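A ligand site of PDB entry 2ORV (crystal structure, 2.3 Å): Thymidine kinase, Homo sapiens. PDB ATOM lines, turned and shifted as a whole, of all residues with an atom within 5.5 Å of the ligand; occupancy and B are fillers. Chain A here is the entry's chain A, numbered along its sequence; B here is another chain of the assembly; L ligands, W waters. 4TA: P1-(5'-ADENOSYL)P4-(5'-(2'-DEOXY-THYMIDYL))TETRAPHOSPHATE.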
ATOM      1  N   PRO A  27       9.341 -10.647 -13.173  1.00  0.00           N
ATOM      2  CA  PRO A  27       7.962 -10.268 -12.839  1.00  0.00           C
ATOM      3  C   PRO A  27       7.932  -8.849 -12.249  1.00  0.00           C
ATOM      4  O   PRO A  27       8.999  -8.165 -12.143  1.00  0.00           O
ATOM      5  CB  PRO A  27       7.547 -11.308 -11.809  1.00  0.00           C
ATOM      6  CG  PRO A  27       8.838 -11.877 -11.231  1.00  0.00           C
ATOM      7  CD  PRO A  27       9.947 -11.599 -12.198  1.00  0.00           C
ATOM      8  N   MET A  28       6.747  -8.355 -11.902  1.00  0.00           N
ATOM      9  CA  MET A  28       6.650  -7.113 -11.145  1.00  0.00           C
ATOM     10  C   MET A  28       7.305  -7.360  -9.768  1.00  0.00           C
ATOM     11  O   MET A  28       7.370  -8.519  -9.338  1.00  0.00           O
ATOM     12  CB  MET A  28       5.178  -6.745 -10.932  1.00  0.00           C
ATOM     13  CG  MET A  28       4.536  -6.064 -12.145  1.00  0.00           C
ATOM     14  SD  MET A  28       2.833  -5.480 -11.870  1.00  0.00           S
ATOM     15  CE  MET A  28       3.070  -4.124 -10.740  1.00  0.00           C
ATOM     16  N   PHE A  29       7.760  -6.286  -9.098  1.00  0.00           N
ATOM     17  CA  PHE A  29       8.397  -6.338  -7.783  1.00  0.00           C
ATOM     18  C   PHE A  29       9.746  -7.040  -7.729  1.00  0.00           C
ATOM     19  O   PHE A  29      10.164  -7.443  -6.659  1.00  0.00           O
ATOM     20  CB  PHE A  29       7.428  -6.901  -6.717  1.00  0.00           C
ATOM     21  CG  PHE A  29       6.039  -6.324  -6.829  1.00  0.00           C
ATOM     22  CD1 PHE A  29       4.967  -7.119  -7.276  1.00  0.00           C
ATOM     23  CD2 PHE A  29       5.819  -4.967  -6.569  1.00  0.00           C
ATOM     24  CE1 PHE A  29       3.672  -6.572  -7.430  1.00  0.00           C
ATOM     25  CE2 PHE A  29       4.529  -4.387  -6.741  1.00  0.00           C
ATOM     26  CZ  PHE A  29       3.453  -5.198  -7.155  1.00  0.00           C
ATOM     27  N   SER A  30      10.423  -7.215  -8.846  1.00  0.00           N
ATOM     28  CA  SER A  30      11.704  -7.903  -8.821  1.00  0.00           C
ATOM     29  C   SER A  30      12.900  -6.953  -8.879  1.00  0.00           C
ATOM     30  O   SER A  30      14.051  -7.422  -8.928  1.00  0.00           O
ATOM     31  CB  SER A  30      11.800  -8.894  -9.956  1.00  0.00           C
ATOM     32  OG  SER A  30      11.617  -8.252 -11.202  1.00  0.00           O
ATOM     33  N   GLY A  31      12.660  -5.644  -8.908  1.00  0.00           N
ATOM     34  CA  GLY A  31      13.766  -4.658  -8.884  1.00  0.00           C
ATOM     35  C   GLY A  31      14.409  -4.351 -10.230  1.00  0.00           C
ATOM     36  O   GLY A  31      15.557  -3.854 -10.287  1.00  0.00           O
ATOM     37  N   LYS A  32      13.686  -4.603 -11.315  1.00  0.00           N
ATOM     38  CA  LYS A  32      14.230  -4.361 -12.667  1.00  0.00           C
ATOM     39  C   LYS A  32      14.745  -2.958 -12.908  1.00  0.00           C
ATOM     40  O   LYS A  32      15.718  -2.767 -13.656  1.00  0.00           O
ATOM     41  CB  LYS A  32      13.217  -4.726 -13.766  1.00  0.00           C
ATOM     42  CG  LYS A  32      12.468  -6.115 -13.526  1.00  0.00           C
ATOM     43  CD  LYS A  32      11.478  -6.401 -14.654  1.00  0.00           C
ATOM     44  CE  LYS A  32      10.264  -5.491 -14.565  1.00  0.00           C
ATOM     45  NZ  LYS A  32       9.560  -5.822 -13.286  1.00  0.00           N
ATOM     46  N   SER A  33      14.096  -1.971 -12.269  1.00  0.00           N
ATOM     47  CA  SER A  33      14.439  -0.559 -12.402  1.00  0.00           C
ATOM     48  C   SER A  33      15.697  -0.232 -11.622  1.00  0.00           C
ATOM     49  O   SER A  33      16.525   0.555 -12.096  1.00  0.00           O
ATOM     50  CB  SER A  33      13.333   0.330 -11.805  1.00  0.00           C
ATOM     51  OG  SER A  33      12.368   0.585 -12.771  1.00  0.00           O
ATOM     52  N   THR A  34      15.806  -0.787 -10.419  1.00  0.00           N
ATOM     53  CA  THR A  34      16.992  -0.617  -9.624  1.00  0.00           C
ATOM     54  C   THR A  34      18.207  -1.178 -10.357  1.00  0.00           C
ATOM     55  O   THR A  34      19.213  -0.457 -10.532  1.00  0.00           O
ATOM     56  CB  THR A  34      16.892  -1.296  -8.274  1.00  0.00           C
ATOM     57  OG1 THR A  34      15.736  -0.795  -7.594  1.00  0.00           O
ATOM     58  CG2 THR A  34      18.122  -1.002  -7.468  1.00  0.00           C
ATOM     59  N   ASP A  58       2.960   5.863 -16.792  1.00  0.00           N
ATOM     60  CA  ASP A  58       3.100   5.210 -15.501  1.00  0.00           C
ATOM     61  C   ASP A  58       3.714   6.176 -14.502  1.00  0.00           C
ATOM     62  O   ASP A  58       4.944   6.264 -14.355  1.00  0.00           O
ATOM     63  CB  ASP A  58       3.899   3.904 -15.578  1.00  0.00           C
ATOM     64  CG  ASP A  58       3.718   3.024 -14.325  1.00  0.00           C
ATOM     65  OD1 ASP A  58       3.569   3.554 -13.199  1.00  0.00           O
ATOM     66  OD2 ASP A  58       3.709   1.788 -14.463  1.00  0.00           O
ATOM     67  N   ARG A  60       3.273   6.386 -10.934  1.00  0.00           N
ATOM     68  CA  ARG A  60       2.909   5.948  -9.601  1.00  0.00           C
ATOM     69  C   ARG A  60       4.128   6.029  -8.662  1.00  0.00           C
ATOM     70  O   ARG A  60       4.075   5.603  -7.508  1.00  0.00           O
ATOM     71  CB  ARG A  60       2.189   4.568  -9.637  1.00  0.00           C
ATOM     72  CG  ARG A  60       3.071   3.405  -9.944  1.00  0.00           C
ATOM     73  CD  ARG A  60       2.392   2.285 -10.703  1.00  0.00           C
ATOM     74  NE  ARG A  60       3.449   1.585 -11.447  1.00  0.00           N
ATOM     75  CZ  ARG A  60       4.272   0.649 -10.957  1.00  0.00           C
ATOM     76  NH1 ARG A  60       4.159   0.202  -9.699  1.00  0.00           N
ATOM     77  NH2 ARG A  60       5.220   0.148 -11.739  1.00  0.00           N
ATOM     78  N   ASP A  97      13.204   2.186 -19.135  1.00  0.00           N
ATOM     79  CA  ASP A  97      12.384   1.584 -18.127  1.00  0.00           C
ATOM     80  C   ASP A  97      11.035   1.177 -18.720  1.00  0.00           C
ATOM     81  O   ASP A  97      10.626   1.669 -19.776  1.00  0.00           O
ATOM     82  CB  ASP A  97      12.214   2.513 -16.937  1.00  0.00           C
ATOM     83  CG  ASP A  97      11.644   1.776 -15.726  1.00  0.00           C
ATOM     84  OD1 ASP A  97      12.231   0.740 -15.364  1.00  0.00           O
ATOM     85  OD2 ASP A  97      10.612   2.202 -15.141  1.00  0.00           O
ATOM     86  N   GLU A  98      10.367   0.234 -18.039  1.00  0.00           N
ATOM     87  CA  GLU A  98       9.091  -0.393 -18.499  1.00  0.00           C
ATOM     88  C   GLU A  98       8.978  -0.665 -20.005  1.00  0.00           C
ATOM     89  O   GLU A  98       7.954  -0.361 -20.614  1.00  0.00           O
ATOM     90  CB  GLU A  98       7.880   0.429 -18.032  1.00  0.00           C
ATOM     91  CG  GLU A  98       7.835   0.738 -16.546  1.00  0.00           C
ATOM     92  CD  GLU A  98       6.428   1.026 -16.033  1.00  0.00           C
ATOM     93  OE1 GLU A  98       5.530   1.228 -16.857  1.00  0.00           O
ATOM     94  OE2 GLU A  98       6.198   1.019 -14.794  1.00  0.00           O
ATOM     95  N   GLN A 100       8.196  -2.778 -22.011  1.00  0.00           N
ATOM     96  CA  GLN A 100       7.107  -3.528 -22.622  1.00  0.00           C
ATOM     97  C   GLN A 100       6.029  -2.615 -23.197  1.00  0.00           C
ATOM     98  O   GLN A 100       5.157  -3.068 -23.972  1.00  0.00           O
ATOM     99  CB  GLN A 100       6.478  -4.514 -21.638  1.00  0.00           C
ATOM    100  CG  GLN A 100       5.702  -3.878 -20.471  1.00  0.00           C
ATOM    101  CD  GLN A 100       6.613  -3.484 -19.307  1.00  0.00           C
ATOM    102  OE1 GLN A 100       7.815  -3.646 -19.389  1.00  0.00           O
ATOM    103  NE2 GLN A 100       6.033  -2.991 -18.214  1.00  0.00           N
ATOM    104  N   PHE A 101       6.063  -1.343 -22.790  1.00  0.00           N
ATOM    105  CA  PHE A 101       5.022  -0.413 -23.198  1.00  0.00           C
ATOM    106  C   PHE A 101       5.330   0.330 -24.512  1.00  0.00           C
ATOM    107  O   PHE A 101       4.466   0.996 -25.045  1.00  0.00           O
ATOM    108  CB  PHE A 101       4.651   0.507 -22.059  1.00  0.00           C
ATOM    109  CG  PHE A 101       3.762  -0.146 -21.015  1.00  0.00           C
ATOM    110  CD1 PHE A 101       4.092  -0.116 -19.675  1.00  0.00           C
ATOM    111  CD2 PHE A 101       2.575  -0.796 -21.383  1.00  0.00           C
ATOM    112  CE1 PHE A 101       3.272  -0.716 -18.697  1.00  0.00           C
ATOM    113  CE2 PHE A 101       1.723  -1.408 -20.401  1.00  0.00           C
ATOM    114  CZ  PHE A 101       2.069  -1.356 -19.075  1.00  0.00           C
ATOM    115  N   ALA A 122      15.016  -2.436 -18.973  1.00  0.00           N
ATOM    116  CA  ALA A 122      14.207  -3.123 -17.972  1.00  0.00           C
ATOM    117  C   ALA A 122      12.849  -3.298 -18.603  1.00  0.00           C
ATOM    118  O   ALA A 122      12.365  -2.391 -19.290  1.00  0.00           O
ATOM    119  CB  ALA A 122      14.089  -2.311 -16.688  1.00  0.00           C
ATOM    120  N   ALA A 123      12.242  -4.463 -18.399  1.00  0.00           N
ATOM    121  CA  ALA A 123      10.926  -4.793 -18.961  1.00  0.00           C
ATOM    122  C   ALA A 123      10.417  -6.097 -18.354  1.00  0.00           C
ATOM    123  O   ALA A 123      11.180  -6.994 -18.044  1.00  0.00           O
ATOM    124  CB  ALA A 123      11.012  -4.962 -20.474  1.00  0.00           C
ATOM    125  N   LEU A 124       9.107  -6.169 -18.241  1.00  0.00           N
ATOM    126  CA  LEU A 124       8.377  -7.352 -17.883  1.00  0.00           C
ATOM    127  C   LEU A 124       8.345  -8.265 -19.107  1.00  0.00           C
ATOM    128  O   LEU A 124       8.010  -7.832 -20.232  1.00  0.00           O
ATOM    129  CB  LEU A 124       6.945  -6.932 -17.605  1.00  0.00           C
ATOM    130  CG  LEU A 124       6.210  -6.972 -16.307  1.00  0.00           C
ATOM    131  CD1 LEU A 124       7.093  -7.072 -15.137  1.00  0.00           C
ATOM    132  CD2 LEU A 124       5.273  -5.782 -16.201  1.00  0.00           C
ATOM    133  N   GLY A 126       6.351 -11.257 -19.249  1.00  0.00           N
ATOM    134  CA  GLY A 126       4.980 -11.676 -19.428  1.00  0.00           C
ATOM    135  C   GLY A 126       3.892 -10.775 -18.820  1.00  0.00           C
ATOM    136  O   GLY A 126       4.078 -10.110 -17.798  1.00  0.00           O
ATOM    137  N   THR A 127       2.717 -10.798 -19.451  1.00  0.00           N
ATOM    138  CA  THR A 127       1.506 -10.155 -18.945  1.00  0.00           C
ATOM    139  C   THR A 127       1.013 -10.884 -17.698  1.00  0.00           C
ATOM    140  O   THR A 127       1.685 -11.791 -17.178  1.00  0.00           O
ATOM    141  CB  THR A 127       0.379 -10.125 -20.013  1.00  0.00           C
ATOM    142  OG1 THR A 127      -0.126 -11.469 -20.225  1.00  0.00           O
ATOM    143  CG2 THR A 127       0.883  -9.560 -21.346  1.00  0.00           C
ATOM    144  N   PHE A 128      -0.157 -10.469 -17.216  1.00  0.00           N
ATOM    145  CA  PHE A 128      -0.825 -11.092 -16.050  1.00  0.00           C
ATOM    146  C   PHE A 128      -1.289 -12.519 -16.402  1.00  0.00           C
ATOM    147  O   PHE A 128      -1.722 -13.294 -15.541  1.00  0.00           O
ATOM    148  CB  PHE A 128      -2.033 -10.202 -15.608  1.00  0.00           C
ATOM    149  CG  PHE A 128      -3.213 -10.237 -16.569  1.00  0.00           C
ATOM    150  CD1 PHE A 128      -4.360 -10.962 -16.262  1.00  0.00           C
ATOM    151  CD2 PHE A 128      -3.170  -9.568 -17.787  1.00  0.00           C
ATOM    152  CE1 PHE A 128      -5.437 -11.011 -17.143  1.00  0.00           C
ATOM    153  CE2 PHE A 128      -4.257  -9.627 -18.703  1.00  0.00           C
ATOM    154  CZ  PHE A 128      -5.388 -10.337 -18.368  1.00  0.00           C
ATOM    155  N   GLN A 129      -1.222 -12.813 -17.705  1.00  0.00           N
ATOM    156  CA  GLN A 129      -1.659 -14.081 -18.314  1.00  0.00           C
ATOM    157  C   GLN A 129      -0.479 -14.909 -18.736  1.00  0.00           C
ATOM    158  O   GLN A 129      -0.650 -15.983 -19.325  1.00  0.00           O
ATOM    159  CB  GLN A 129      -2.496 -13.822 -19.572  1.00  0.00           C
ATOM    160  CG  GLN A 129      -3.914 -13.403 -19.280  1.00  0.00           C
ATOM    161  CD  GLN A 129      -4.680 -12.920 -20.501  1.00  0.00           C
ATOM    162  OE1 GLN A 129      -5.911 -13.055 -20.521  1.00  0.00           O
ATOM    163  NE2 GLN A 129      -3.997 -12.350 -21.513  1.00  0.00           N
ATOM    164  N   PHE A 133       4.762  -9.774 -23.531  1.00  0.00           N
ATOM    165  CA  PHE A 133       4.256  -8.429 -23.250  1.00  0.00           C
ATOM    166  C   PHE A 133       4.854  -7.507 -24.266  1.00  0.00           C
ATOM    167  O   PHE A 133       6.048  -7.187 -24.202  1.00  0.00           O
ATOM    168  CB  PHE A 133       4.701  -7.985 -21.855  1.00  0.00           C
ATOM    169  CG  PHE A 133       3.813  -6.945 -21.207  1.00  0.00           C
ATOM    170  CD1 PHE A 133       3.657  -6.934 -19.826  1.00  0.00           C
ATOM    171  CD2 PHE A 133       3.154  -5.959 -21.964  1.00  0.00           C
ATOM    172  CE1 PHE A 133       2.875  -5.969 -19.211  1.00  0.00           C
ATOM    173  CE2 PHE A 133       2.358  -4.993 -21.363  1.00  0.00           C
ATOM    174  CZ  PHE A 133       2.215  -5.001 -19.984  1.00  0.00           C
ATOM    175  N   THR A 163       3.596 -12.551 -12.560  1.00  0.00           N
ATOM    176  CA  THR A 163       2.668 -11.585 -11.980  1.00  0.00           C
ATOM    177  C   THR A 163       1.191 -11.987 -12.223  1.00  0.00           C
ATOM    178  O   THR A 163       0.787 -12.202 -13.360  1.00  0.00           O
ATOM    179  CB  THR A 163       2.884 -10.151 -12.558  1.00  0.00           C
ATOM    180  OG1 THR A 163       4.277  -9.879 -12.721  1.00  0.00           O
ATOM    181  CG2 THR A 163       2.265  -9.110 -11.613  1.00  0.00           C
ATOM    182  N   ARG A 165      -2.883 -10.779 -11.741  1.00  0.00           N
ATOM    183  CA  ARG A 165      -3.808  -9.645 -11.552  1.00  0.00           C
ATOM    184  C   ARG A 165      -4.889 -10.048 -10.541  1.00  0.00           C
ATOM    185  O   ARG A 165      -5.562 -11.064 -10.717  1.00  0.00           O
ATOM    186  CB  ARG A 165      -4.440  -9.265 -12.880  1.00  0.00           C
ATOM    187  CG  ARG A 165      -5.404  -8.089 -12.864  1.00  0.00           C
ATOM    188  CD  ARG A 165      -5.883  -7.781 -14.272  1.00  0.00           C
ATOM    189  NE  ARG A 165      -4.866  -7.012 -14.975  1.00  0.00           N
ATOM    190  CZ  ARG A 165      -4.935  -6.601 -16.235  1.00  0.00           C
ATOM    191  NH1 ARG A 165      -5.974  -6.871 -17.006  1.00  0.00           N
ATOM    192  NH2 ARG A 165      -3.927  -5.915 -16.734  1.00  0.00           N
ATOM    193  N   VAL A 172      -4.928  -5.726 -21.552  1.00  0.00           N
ATOM    194  CA  VAL A 172      -3.540  -5.938 -21.183  1.00  0.00           C
ATOM    195  C   VAL A 172      -3.035  -4.815 -20.255  1.00  0.00           C
ATOM    196  O   VAL A 172      -2.587  -5.108 -19.131  1.00  0.00           O
ATOM    197  CB  VAL A 172      -2.639  -6.212 -22.426  1.00  0.00           C
ATOM    198  CG1 VAL A 172      -1.217  -5.690 -22.260  1.00  0.00           C
ATOM    199  CG2 VAL A 172      -2.640  -7.707 -22.746  1.00  0.00           C
ATOM    200  N   GLU A 173      -3.181  -3.538 -20.675  1.00  0.00           N
ATOM    201  CA  GLU A 173      -2.617  -2.373 -19.950  1.00  0.00           C
ATOM    202  C   GLU A 173      -3.518  -1.824 -18.834  1.00  0.00           C
ATOM    203  O   GLU A 173      -4.533  -1.231 -19.088  1.00  0.00           O
ATOM    204  CB  GLU A 173      -2.137  -1.242 -20.907  1.00  0.00           C
ATOM    205  CG  GLU A 173      -1.666   0.062 -20.200  1.00  0.00           C
ATOM    206  CD  GLU A 173      -0.867   1.005 -21.091  1.00  0.00           C
ATOM    207  OE1 GLU A 173      -0.533   2.132 -20.651  1.00  0.00           O
ATOM    208  OE2 GLU A 173      -0.547   0.626 -22.248  1.00  0.00           O
ATOM    209  N   VAL A 174      -3.109  -2.061 -17.607  1.00  0.00           N
ATOM    210  CA  VAL A 174      -3.732  -1.486 -16.445  1.00  0.00           C
ATOM    211  C   VAL A 174      -2.562  -1.115 -15.524  1.00  0.00           C
ATOM    212  O   VAL A 174      -1.980  -1.973 -14.876  1.00  0.00           O
ATOM    213  CB  VAL A 174      -4.708  -2.462 -15.765  1.00  0.00           C
ATOM    214  CG1 VAL A 174      -5.198  -1.929 -14.414  1.00  0.00           C
ATOM    215  CG2 VAL A 174      -5.882  -2.771 -16.674  1.00  0.00           C
ATOM    216  N   ILE A 175      -2.221   0.178 -15.523  1.00  0.00           N
ATOM    217  CA  ILE A 175      -1.201   0.731 -14.629  1.00  0.00           C
ATOM    218  C   ILE A 175      -1.644   0.506 -13.192  1.00  0.00           C
ATOM    219  O   ILE A 175      -2.797   0.706 -12.881  1.00  0.00           O
ATOM    220  CB  ILE A 175      -0.949   2.258 -14.930  1.00  0.00           C
ATOM    221  CG1 ILE A 175      -0.610   2.494 -16.418  1.00  0.00           C
ATOM    222  CG2 ILE A 175       0.048   2.914 -13.929  1.00  0.00           C
ATOM    223  CD1 ILE A 175       0.549   1.697 -17.002  1.00  0.00           C
ATOM    224  N   GLY A 176      -0.724   0.053 -12.331  1.00  0.00           N
ATOM    225  CA  GLY A 176      -1.012  -0.192 -10.913  1.00  0.00           C
ATOM    226  C   GLY A 176       0.130  -0.907 -10.195  1.00  0.00           C
ATOM    227  O   GLY A 176       1.118  -1.306 -10.820  1.00  0.00           O
ATOM    228  N   GLY A 177      -0.007  -1.044  -8.880  1.00  0.00           N
ATOM    229  CA  GLY A 177       1.011  -1.624  -8.019  1.00  0.00           C
ATOM    230  C   GLY A 177       0.468  -2.803  -7.232  1.00  0.00           C
ATOM    231  O   GLY A 177      -0.402  -3.522  -7.721  1.00  0.00           O
ATOM    232  N   TYR A 181      -1.914  -6.017  -8.384  1.00  0.00           N
ATOM    233  CA  TYR A 181      -1.099  -7.184  -8.780  1.00  0.00           C
ATOM    234  C   TYR A 181      -0.319  -7.845  -7.637  1.00  0.00           C
ATOM    235  O   TYR A 181       0.100  -7.175  -6.683  1.00  0.00           O
ATOM    236  CB  TYR A 181      -0.080  -6.746  -9.810  1.00  0.00           C
ATOM    237  CG  TYR A 181      -0.633  -6.196 -11.101  1.00  0.00           C
ATOM    238  CD1 TYR A 181      -0.779  -4.816 -11.292  1.00  0.00           C
ATOM    239  CD2 TYR A 181      -0.928  -7.030 -12.158  1.00  0.00           C
ATOM    240  CE1 TYR A 181      -1.257  -4.309 -12.507  1.00  0.00           C
ATOM    241  CE2 TYR A 181      -1.397  -6.527 -13.383  1.00  0.00           C
ATOM    242  CZ  TYR A 181      -1.544  -5.178 -13.532  1.00  0.00           C
ATOM    243  OH  TYR A 181      -2.002  -4.718 -14.730  1.00  0.00           O
ATOM    244  N   ILE B  45       8.499  -5.371   0.255  1.00  0.00           N
ATOM    245  CA  ILE B  45       7.235  -5.206  -0.451  1.00  0.00           C
ATOM    246  C   ILE B  45       6.351  -6.471  -0.303  1.00  0.00           C
ATOM    247  O   ILE B  45       5.203  -6.501  -0.747  1.00  0.00           O
ATOM    248  CB  ILE B  45       7.480  -4.878  -1.931  1.00  0.00           C
ATOM    249  CG1 ILE B  45       6.181  -4.430  -2.629  1.00  0.00           C
ATOM    250  CG2 ILE B  45       8.089  -6.059  -2.651  1.00  0.00           C
ATOM    251  CD1 ILE B  45       6.125  -2.956  -2.963  1.00  0.00           C
HETATM  252  C5M 4TA L   1       1.454  -7.786 -15.608  1.00  0.00           C
HETATM  253  C5  4TA L   1       0.994  -6.467 -16.173  1.00  0.00           C
HETATM  254  C6  4TA L   1       1.477  -5.288 -15.637  1.00  0.00           C
HETATM  255  N1  4TA L   1       1.077  -4.112 -16.121  1.00  0.00           N
HETATM  256  C1B 4TA L   1       1.586  -2.827 -15.572  1.00  0.00           C
HETATM  257  C2B 4TA L   1       1.337  -2.702 -14.082  1.00  0.00           C
HETATM  258  C3B 4TA L   1       2.362  -1.638 -13.733  1.00  0.00           C
HETATM  259  O3B 4TA L   1       1.810  -0.333 -13.827  1.00  0.00           O
HETATM  260  C4B 4TA L   1       3.466  -1.723 -14.762  1.00  0.00           C
HETATM  261  C5B 4TA L   1       4.657  -2.276 -13.963  1.00  0.00           C
HETATM  262  O5' 4TA L   1       5.657  -2.814 -14.803  1.00  0.00           O
HETATM  263  PD  4TA L   1       7.180  -3.015 -14.284  1.00  0.00           P
HETATM  264  O2D 4TA L   1       8.050  -3.041 -15.642  1.00  0.00           O
HETATM  265  O1D 4TA L   1       7.259  -4.412 -13.270  1.00  0.00           O
HETATM  266  OCD 4TA L   1       7.471  -1.713 -13.403  1.00  0.00           O
HETATM  267  PC  4TA L   1       8.880  -1.258 -12.795  1.00  0.00           P
HETATM  268  O1C 4TA L   1       9.980  -0.518 -13.978  1.00  0.00           O
HETATM  269  O2C 4TA L   1       8.593  -0.200 -11.671  1.00  0.00           O
HETATM  270  OBC 4TA L   1       9.376  -2.696 -12.221  1.00  0.00           O
HETATM  271  PB  4TA L   1      10.284  -2.976 -10.938  1.00  0.00           P
HETATM  272  O2B 4TA L   1      10.767  -4.673 -10.915  1.00  0.00           O
HETATM  273  O1B 4TA L   1      11.457  -1.891 -11.060  1.00  0.00           O
HETATM  274  OAB 4TA L   1       9.299  -2.769  -9.686  1.00  0.00           O
HETATM  275  PA  4TA L   1       9.780  -2.520  -8.162  1.00  0.00           P
HETATM  276  O1A 4TA L   1      10.715  -1.213  -8.010  1.00  0.00           O
HETATM  277  O2A 4TA L   1       8.338  -2.425  -7.097  1.00  0.00           O
HETATM  278  OA  4TA L   1      10.544  -3.857  -7.741  1.00  0.00           O
HETATM  279  O4' 4TA L   1       2.977  -2.559 -15.806  1.00  0.00           O
HETATM  280  C2  4TA L   1       0.141  -4.055 -17.183  1.00  0.00           C
HETATM  281  O2  4TA L   1      -0.201  -2.933 -17.632  1.00  0.00           O
HETATM  282  N3  4TA L   1      -0.361  -5.170 -17.721  1.00  0.00           N
HETATM  283  C4  4TA L   1       0.004  -6.391 -17.292  1.00  0.00           C
HETATM  284  O4  4TA L   1      -0.491  -7.436 -17.801  1.00  0.00           O
HETATM  285  O   HOH W   1      11.283  -0.495  -5.410  1.00  0.00           O
HETATM  286  O   HOH W   2       9.810   2.304 -12.613  1.00  0.00           O
HETATM  287  O   HOH W   3       7.003  -3.535 -11.040  1.00  0.00           O
HETATM  288  O   HOH W   4      12.876  -1.090  -9.208  1.00  0.00           O
HETATM  289  O   HOH W   5      11.006  -4.918  -5.367  1.00  0.00           O
HETATM  290  O   HOH W   6       9.439  -2.941  -4.548  1.00  0.00           O
HETATM  291  O   HOH W   7      10.851  -2.113 -16.174  1.00  0.00           O
HETATM  292  O   HOH W   8       7.518  -0.910  -5.093  1.00  0.00           O
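The backbone carbonyl oxygen (O) of Val 172 is in hydrogen-bond range of a nitrogen (N3) of the ligand, 2.6 Å away.
The backbone NH (N) of Lys 32 lies within hydrogen-bond range of an oxygen (O2B) of the ligand (2.9 Å).
NZ of Lys 32 lies within salt-bridge range of O1D of the ligand (2.7 Å).
N of Ser 33 is in hydrogen-bond range of O1B of the ligand.
OG of Ser 33 lies within hydrogen-bond range of O1C of the ligand (2.9 Å).
The side-chain carboxylate of Asp 58 is in hydrogen-bond range of an oxygen (O3B) of the ligand.
The backbone NH (N) of Gly 31 sits at hydrogen-bond distance from an oxygen (O2B) of the ligand (2.9 Å).
The side-chain carboxylate (OD1) of Asp 97 sits close to an oxygen (O1C) of the ligand.
O3B of the ligand sits at hydrogen-bond distance from N of Gly 176, 3.0 Å away.
O3B of the ligand sits close to O of Gly 176, 3.2 Å away.
N of Val 174 lies within hydrogen-bond range of O2 of the ligand.
N of Phe 128 sits at hydrogen-bond distance from O4 of the ligand (3.1 Å).
NE2 of Gln 100 is in hydrogen-bond range of O2D of the ligand, 3.3 Å away.
An oxygen (O2B) of the ligand sits at hydrogen-bond distance from the backbone NH (N) of Ser 30 (3.3 Å).
A nitrogen (N3) of the ligand sits close to the side-chain hydroxyl (OH) of Tyr 181 (3.4 Å).
O2C of the ligand is in salt-bridge range of NH2 of Arg 60, 3.4 Å away.
The backbone carbonyl oxygen (O) of Val 172 lies within hydrogen-bond range of the guanidinium group (NH2) of Arg 165, at 2.9 Å.
NZ of Lys 32 sits at hydrogen-bond distance from O of Pro 27.
The side-chain hydroxyl (OG) of Ser 33 sits at hydrogen-bond distance from the side-chain carboxylate (OD1) of Asp 97, at 2.6 Å.
The side-chain carboxylate (OD2) of Asp 58 lies close to the side-chain carboxylate (OE2) of Glu 98 (2.6 Å).
The backbone carbonyl oxygen of Val 174 lies within hydrogen-bond range of the side-chain hydroxyl of Tyr 181, at 2.7 Å.
The side-chain amide oxygen of Gln 100 lies within hydrogen-bond range of the backbone NH of Leu 124 (3.1 Å).
The backbone NH of Met 28 sits at hydrogen-bond distance from the side-chain hydroxyl of Thr 163.
OG1 of Thr 127 lies close to N of Gln 129.
OE2 of Glu 98 lies close to OCD of the ligand (3.3 Å).
Merely in contact with the ligand: Met 28, Phe 29, Phe 101, Leu 124, Thr 127, Phe 133, Arg 165, Glu 173 and Ile 175.
Hydrophobic or aromatic side chains within 4 Å of the ligand: Met 28, Phe 29, Phe 101, Leu 124, Phe 128, Phe 133, Ile 175 and Tyr 181.
Along chain A the residues within 4 Å of the ligand span positions 28 to 181.
The nearest printed residue that does not touch the ligand is Pro 27 (4.1 Å).
Water W3 bridges O1D of the ligand (2.4 Å) and N of Phe 29 (3.5 Å).
Water W4 lies within hydrogen-bond range of an oxygen (O1B) of the ligand (2.5 Å), the backbone NH (N) of Thr 34 (3.2 Å) and the backbone NH (N) of Ser 33 (3.4 Å).
Water W5 bridges OA of the ligand (2.6 Å) and O of Phe 29 (3.0 Å).
Water W7 lies within hydrogen-bond range of O1C of the ligand (2.9 Å), N of Glu 98 (3.0 Å), OD1 of Asp 97 (3.3 Å) and O of Ala 122 (3.5 Å).
Water W2 lies within hydrogen-bond range of the side-chain carboxylate of Asp 97 (2.7 Å), an oxygen (O2C) of the ligand (2.9 Å) and the side-chain hydroxyl of Ser 33 (3.1 Å).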
